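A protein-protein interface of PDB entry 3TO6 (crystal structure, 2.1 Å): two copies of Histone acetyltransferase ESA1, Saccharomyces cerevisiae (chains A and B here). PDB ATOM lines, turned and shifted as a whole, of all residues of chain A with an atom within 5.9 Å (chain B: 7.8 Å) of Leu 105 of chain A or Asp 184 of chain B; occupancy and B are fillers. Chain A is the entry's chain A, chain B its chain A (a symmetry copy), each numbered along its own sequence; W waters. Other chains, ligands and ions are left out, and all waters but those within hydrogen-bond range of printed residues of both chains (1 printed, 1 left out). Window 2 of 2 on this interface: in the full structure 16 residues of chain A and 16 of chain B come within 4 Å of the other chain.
Of the 8 printed residues of chain A, 4 touch a printed residue of chain B. Hydrophobic or aromatic side chains of chain A that line the printed part of chain B: Pro 25, Leu 105 and Tyr 106. Along chain A the printed residues that touch a printed residue of chain B span positions 25 to 108. Of the 11 printed residues of chain B, 5 touch a printed residue of chain A. Hydrophobic or aromatic side chains of chain B within 4 Å of the printed part of chain A: Leu 185, Leu 187 and Leu 188. Among the printed residues, Asp or Glu carboxylates within 4 Å of a Lys or Arg side-chain nitrogen of the other chain: Asp 108 of chain A with Arg 191 of chain B (2.7 Å).
N of Tyr 106 of chain A is in hydrogen-bond range of OD2 of Asp 184 of chain B, 3.2 Å away. The side-chain carboxylate of Asp 108 of chain A lies within salt-bridge range of the guanidinium group of Arg 191 of chain B (2.7 Å).
O of Leu 185 of chain B is in hydrogen-bond range of OG of Ser 189 of chain B (3.5 Å).
Leu 105 of chain A touches just these residues of chain B: Asp 184 (3.4 Å), Leu 187 (3.7 Å) and Arg 191 (3.6 Å). Asp 184 of chain B touches just these residues of chain A: Pro 25 (3.8 Å), Leu 105 (3.4 Å) and Tyr 106 (3.2 Å). No residue of chain B comes within 4 Å of Thr 104 of chain A. Printed residues of chain A within 4 Å of Arg 191 of chain B: Leu 105 (3.6 Å) and Asp 108 (2.7 Å). Of the printed residues of chain B, Asp 108 of chain A touches Arg 191 (2.7 Å). Printed residues of chain B within 4 Å of Pro 25 of chain A: Asp 184 and Leu 185. Tyr 107 of chain A touches none of the printed residues of chain B. The nearest residue of chain A that does not touch Asp 184 of chain B is Thr 104 of chain A (4.3 Å). The nearest printed residue of chain B that does not touch Tyr 106 of chain A is Leu 185 of chain B (6.2 Å).
No position is printed for both chains.
Water W1 bridges O of ALY 103 of chain A and the side-chain carboxylate (OD1) of Asp 184 of chain B.
Among the printed residues, merely in contact across the chains: Pro 25 of chain A with Asp 184 of chain B (3.8 Å), Pro 25 of chain A with Leu 185 of chain B (3.7 Å), Leu 105 of chain A with Asp 184 of chain B (3.4 Å), Leu 105 of chain A with Leu 187 of chain B (3.7 Å), Leu 105 of chain A with Arg 191 of chain B (3.6 Å) and Tyr 106 of chain A with Leu 188 of chain B (3.3 Å).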
ATOM      1  N   PRO A  25       6.908  14.192  -5.725  1.00  0.00           N
ATOM      2  CA  PRO A  25       7.914  15.251  -5.524  1.00  0.00           C
ATOM      3  C   PRO A  25       8.171  15.666  -4.067  1.00  0.00           C
ATOM      4  O   PRO A  25       8.149  16.865  -3.762  1.00  0.00           O
ATOM      5  CB  PRO A  25       7.311  16.432  -6.280  1.00  0.00           C
ATOM      6  CG  PRO A  25       5.810  16.233  -6.094  1.00  0.00           C
ATOM      7  CD  PRO A  25       5.625  14.730  -6.219  1.00  0.00           C
ATOM      8  OH  ALY A 103      -6.218  14.886  -4.145  1.00  0.00           O
ATOM      9  CH  ALY A 103      -5.624  15.849  -4.601  1.00  0.00           C
ATOM     10  CH3 ALY A 103      -6.180  17.239  -4.528  1.00  0.00           C
ATOM     11  NZ  ALY A 103      -4.440  15.733  -5.196  1.00  0.00           N
ATOM     12  CE  ALY A 103      -3.710  14.480  -5.196  1.00  0.00           C
ATOM     13  CD  ALY A 103      -2.538  14.501  -6.169  1.00  0.00           C
ATOM     14  CG  ALY A 103      -3.006  14.229  -7.593  1.00  0.00           C
ATOM     15  CB  ALY A 103      -1.821  14.121  -8.546  1.00  0.00           C
ATOM     16  CA  ALY A 103      -2.171  14.685  -9.918  1.00  0.00           C
ATOM     17  N   ALY A 103      -1.458  13.947 -10.942  1.00  0.00           N
ATOM     18  C   ALY A 103      -1.775  16.131  -9.979  1.00  0.00           C
ATOM     19  O   ALY A 103      -0.634  16.453 -10.265  1.00  0.00           O
ATOM     20  N   THR A 104      -2.730  17.015  -9.709  1.00  0.00           N
ATOM     21  CA  THR A 104      -2.476  18.450  -9.735  1.00  0.00           C
ATOM     22  C   THR A 104      -1.382  18.836  -8.745  1.00  0.00           C
ATOM     23  O   THR A 104      -1.137  18.129  -7.769  1.00  0.00           O
ATOM     24  CB  THR A 104      -3.751  19.254  -9.417  1.00  0.00           C
ATOM     25  OG1 THR A 104      -3.513  20.647  -9.659  1.00  0.00           O
ATOM     26  CG2 THR A 104      -4.155  19.058  -7.965  1.00  0.00           C
ATOM     27  N   LEU A 105      -0.728  19.964  -9.006  1.00  0.00           N
ATOM     28  CA  LEU A 105       0.353  20.453  -8.129  1.00  0.00           C
ATOM     29  C   LEU A 105       0.039  20.288  -6.629  1.00  0.00           C
ATOM     30  O   LEU A 105      -0.893  20.899  -6.120  1.00  0.00           O
ATOM     31  CB  LEU A 105       0.642  21.923  -8.435  1.00  0.00           C
ATOM     32  CG  LEU A 105       1.563  22.661  -7.458  1.00  0.00           C
ATOM     33  CD1 LEU A 105       2.990  22.097  -7.523  1.00  0.00           C
ATOM     34  CD2 LEU A 105       1.566  24.174  -7.746  1.00  0.00           C
ATOM     35  N   TYR A 106       0.828  19.486  -5.922  1.00  0.00           N
ATOM     36  CA  TYR A 106       0.475  19.107  -4.553  1.00  0.00           C
ATOM     37  C   TYR A 106       0.395  20.307  -3.614  1.00  0.00           C
ATOM     38  O   TYR A 106      -0.317  20.277  -2.604  1.00  0.00           O
ATOM     39  CB  TYR A 106       1.476  18.100  -3.980  1.00  0.00           C
ATOM     40  CG  TYR A 106       2.802  18.711  -3.551  1.00  0.00           C
ATOM     41  CD1 TYR A 106       3.003  19.154  -2.251  1.00  0.00           C
ATOM     42  CD2 TYR A 106       3.848  18.842  -4.455  1.00  0.00           C
ATOM     43  CE1 TYR A 106       4.223  19.717  -1.857  1.00  0.00           C
ATOM     44  CE2 TYR A 106       5.052  19.394  -4.086  1.00  0.00           C
ATOM     45  CZ  TYR A 106       5.244  19.829  -2.790  1.00  0.00           C
ATOM     46  OH  TYR A 106       6.472  20.366  -2.454  1.00  0.00           O
ATOM     47  N   TYR A 107       1.135  21.356  -3.951  1.00  0.00           N
ATOM     48  CA  TYR A 107       1.301  22.503  -3.064  1.00  0.00           C
ATOM     49  C   TYR A 107       0.063  23.387  -2.962  1.00  0.00           C
ATOM     50  O   TYR A 107      -0.163  24.024  -1.939  1.00  0.00           O
ATOM     51  CB  TYR A 107       2.487  23.350  -3.541  1.00  0.00           C
ATOM     52  CG  TYR A 107       3.027  24.270  -2.485  1.00  0.00           C
ATOM     53  CD1 TYR A 107       3.911  23.802  -1.532  1.00  0.00           C
ATOM     54  CD2 TYR A 107       2.648  25.607  -2.437  1.00  0.00           C
ATOM     55  CE1 TYR A 107       4.415  24.648  -0.554  1.00  0.00           C
ATOM     56  CE2 TYR A 107       3.147  26.459  -1.466  1.00  0.00           C
ATOM     57  CZ  TYR A 107       4.033  25.971  -0.534  1.00  0.00           C
ATOM     58  OH  TYR A 107       4.537  26.800   0.441  1.00  0.00           O
ATOM     59  N   ASP A 108      -0.729  23.451  -4.026  1.00  0.00           N
ATOM     60  CA  ASP A 108      -1.880  24.347  -4.032  1.00  0.00           C
ATOM     61  C   ASP A 108      -3.142  23.607  -3.551  1.00  0.00           C
ATOM     62  O   ASP A 108      -3.848  22.990  -4.353  1.00  0.00           O
ATOM     63  CB  ASP A 108      -2.082  24.961  -5.429  1.00  0.00           C
ATOM     64  CG  ASP A 108      -0.984  25.989  -5.798  1.00  0.00           C
ATOM     65  OD1 ASP A 108      -0.135  26.317  -4.939  1.00  0.00           O
ATOM     66  OD2 ASP A 108      -0.984  26.483  -6.946  1.00  0.00           O
ATOM     67  N   VAL A 109      -3.405  23.665  -2.242  1.00  0.00           N
ATOM     68  CA  VAL A 109      -4.533  22.946  -1.639  1.00  0.00           C
ATOM     69  C   VAL A 109      -5.762  23.829  -1.365  1.00  0.00           C
ATOM     70  O   VAL A 109      -6.834  23.320  -1.041  1.00  0.00           O
ATOM     71  CB  VAL A 109      -4.122  22.192  -0.339  1.00  0.00           C
ATOM     72  CG1 VAL A 109      -3.137  21.066  -0.653  1.00  0.00           C
ATOM     73  CG2 VAL A 109      -3.530  23.148   0.696  1.00  0.00           C
ATOM     74  N   PRO B 181       2.708  22.351 -19.746  1.00  0.00           N
ATOM     75  CA  PRO B 181       2.686  22.339 -18.283  1.00  0.00           C
ATOM     76  C   PRO B 181       4.064  22.049 -17.707  1.00  0.00           C
ATOM     77  O   PRO B 181       4.885  21.404 -18.380  1.00  0.00           O
ATOM     78  CB  PRO B 181       1.728  21.180 -17.968  1.00  0.00           C
ATOM     79  CG  PRO B 181       1.945  20.233 -19.103  1.00  0.00           C
ATOM     80  CD  PRO B 181       2.152  21.108 -20.314  1.00  0.00           C
ATOM     81  N   LEU B 182       4.316  22.539 -16.492  1.00  0.00           N
ATOM     82  CA  LEU B 182       5.561  22.268 -15.765  1.00  0.00           C
ATOM     83  C   LEU B 182       5.351  21.138 -14.772  1.00  0.00           C
ATOM     84  O   LEU B 182       4.270  21.031 -14.199  1.00  0.00           O
ATOM     85  CB  LEU B 182       6.003  23.498 -14.958  1.00  0.00           C
ATOM     86  CG  LEU B 182       6.627  24.709 -15.659  1.00  0.00           C
ATOM     87  CD1 LEU B 182       5.529  25.589 -16.198  1.00  0.00           C
ATOM     88  CD2 LEU B 182       7.496  25.510 -14.709  1.00  0.00           C
ATOM     89  N   SER B 183       6.385  20.332 -14.531  1.00  0.00           N
ATOM     90  CA  SER B 183       6.374  19.395 -13.409  1.00  0.00           C
ATOM     91  C   SER B 183       6.258  20.175 -12.088  1.00  0.00           C
ATOM     92  O   SER B 183       6.548  21.365 -12.050  1.00  0.00           O
ATOM     93  CB  SER B 183       7.658  18.557 -13.403  1.00  0.00           C
ATOM     94  OG  SER B 183       8.799  19.368 -13.128  1.00  0.00           O
ATOM     95  N   ASP B 184       5.845  19.519 -11.008  1.00  0.00           N
ATOM     96  CA  ASP B 184       5.723  20.195  -9.715  1.00  0.00           C
ATOM     97  C   ASP B 184       7.083  20.746  -9.286  1.00  0.00           C
ATOM     98  O   ASP B 184       7.200  21.878  -8.808  1.00  0.00           O
ATOM     99  CB  ASP B 184       5.202  19.230  -8.625  1.00  0.00           C
ATOM    100  CG  ASP B 184       3.702  18.917  -8.747  1.00  0.00           C
ATOM    101  OD1 ASP B 184       3.074  19.191  -9.802  1.00  0.00           O
ATOM    102  OD2 ASP B 184       3.154  18.382  -7.757  1.00  0.00           O
ATOM    103  N   LEU B 185       8.118  19.928  -9.436  1.00  0.00           N
ATOM    104  CA  LEU B 185       9.477  20.375  -9.114  1.00  0.00           C
ATOM    105  C   LEU B 185       9.874  21.649  -9.890  1.00  0.00           C
ATOM    106  O   LEU B 185      10.421  22.590  -9.319  1.00  0.00           O
ATOM    107  CB  LEU B 185      10.481  19.267  -9.416  1.00  0.00           C
ATOM    108  CG  LEU B 185      11.035  18.308  -8.359  1.00  0.00           C
ATOM    109  CD1 LEU B 185      10.404  18.424  -6.987  1.00  0.00           C
ATOM    110  CD2 LEU B 185      11.081  16.864  -8.872  1.00  0.00           C
ATOM    111  N   GLY B 186       9.608  21.674 -11.188  1.00  0.00           N
ATOM    112  CA  GLY B 186       9.909  22.847 -11.993  1.00  0.00           C
ATOM    113  C   GLY B 186       9.110  24.082 -11.567  1.00  0.00           C
ATOM    114  O   GLY B 186       9.657  25.177 -11.413  1.00  0.00           O
ATOM    115  N   LEU B 187       7.806  23.913 -11.362  1.00  0.00           N
ATOM    116  CA  LEU B 187       6.973  25.066 -11.032  1.00  0.00           C
ATOM    117  C   LEU B 187       7.370  25.670  -9.683  1.00  0.00           C
ATOM    118  O   LEU B 187       7.450  26.896  -9.550  1.00  0.00           O
ATOM    119  CB  LEU B 187       5.484  24.717 -11.069  1.00  0.00           C
ATOM    120  CG  LEU B 187       4.530  25.905 -10.837  1.00  0.00           C
ATOM    121  CD1 LEU B 187       4.812  27.010 -11.841  1.00  0.00           C
ATOM    122  CD2 LEU B 187       3.079  25.469 -10.921  1.00  0.00           C
ATOM    123  N   LEU B 188       7.659  24.825  -8.692  1.00  0.00           N
ATOM    124  CA  LEU B 188       8.093  25.351  -7.395  1.00  0.00           C
ATOM    125  C   LEU B 188       9.450  26.077  -7.492  1.00  0.00           C
ATOM    126  O   LEU B 188       9.679  27.061  -6.793  1.00  0.00           O
ATOM    127  CB  LEU B 188       8.132  24.256  -6.312  1.00  0.00           C
ATOM    128  CG  LEU B 188       6.780  23.619  -5.930  1.00  0.00           C
ATOM    129  CD1 LEU B 188       6.963  22.551  -4.855  1.00  0.00           C
ATOM    130  CD2 LEU B 188       5.794  24.665  -5.460  1.00  0.00           C
ATOM    131  N   SER B 189      10.351  25.591  -8.344  1.00  0.00           N
ATOM    132  CA  SER B 189      11.608  26.300  -8.572  1.00  0.00           C
ATOM    133  C   SER B 189      11.398  27.665  -9.223  1.00  0.00           C
ATOM    134  O   SER B 189      12.009  28.650  -8.804  1.00  0.00           O
ATOM    135  CB  SER B 189      12.575  25.464  -9.429  1.00  0.00           C
ATOM    136  OG  SER B 189      13.208  24.505  -8.613  1.00  0.00           O
ATOM    137  N   TYR B 190      10.566  27.718 -10.264  1.00  0.00           N
ATOM    138  CA  TYR B 190      10.212  29.004 -10.880  1.00  0.00           C
ATOM    139  C   TYR B 190       9.550  29.986  -9.893  1.00  0.00           C
ATOM    140  O   TYR B 190       9.881  31.178  -9.868  1.00  0.00           O
ATOM    141  CB  TYR B 190       9.348  28.813 -12.143  1.00  0.00           C
ATOM    142  CG  TYR B 190      10.177  28.641 -13.409  1.00  0.00           C
ATOM    143  CD1 TYR B 190      10.528  27.369 -13.875  1.00  0.00           C
ATOM    144  CD2 TYR B 190      10.618  29.748 -14.127  1.00  0.00           C
ATOM    145  CE1 TYR B 190      11.297  27.210 -15.017  1.00  0.00           C
ATOM    146  CE2 TYR B 190      11.393  29.600 -15.282  1.00  0.00           C
ATOM    147  CZ  TYR B 190      11.732  28.335 -15.715  1.00  0.00           C
ATOM    148  OH  TYR B 190      12.488  28.193 -16.860  1.00  0.00           O
ATOM    149  N   ARG B 191       8.613  29.504  -9.082  1.00  0.00           N
ATOM    150  CA  ARG B 191       7.962  30.395  -8.131  1.00  0.00           C
ATOM    151  C   ARG B 191       8.972  30.994  -7.152  1.00  0.00           C
ATOM    152  O   ARG B 191       8.874  32.169  -6.810  1.00  0.00           O
ATOM    153  CB  ARG B 191       6.840  29.677  -7.363  1.00  0.00           C
ATOM    154  CG  ARG B 191       5.582  29.400  -8.191  1.00  0.00           C
ATOM    155  CD  ARG B 191       4.524  28.691  -7.324  1.00  0.00           C
ATOM    156  NE  ARG B 191       3.263  28.493  -8.019  1.00  0.00           N
ATOM    157  CZ  ARG B 191       2.205  27.875  -7.492  1.00  0.00           C
ATOM    158  NH1 ARG B 191       2.255  27.387  -6.254  1.00  0.00           N
ATOM    159  NH2 ARG B 191       1.100  27.744  -8.209  1.00  0.00           N
HETATM  160  O   HOH W   1       1.138  18.152 -11.475  1.00  0.00           O
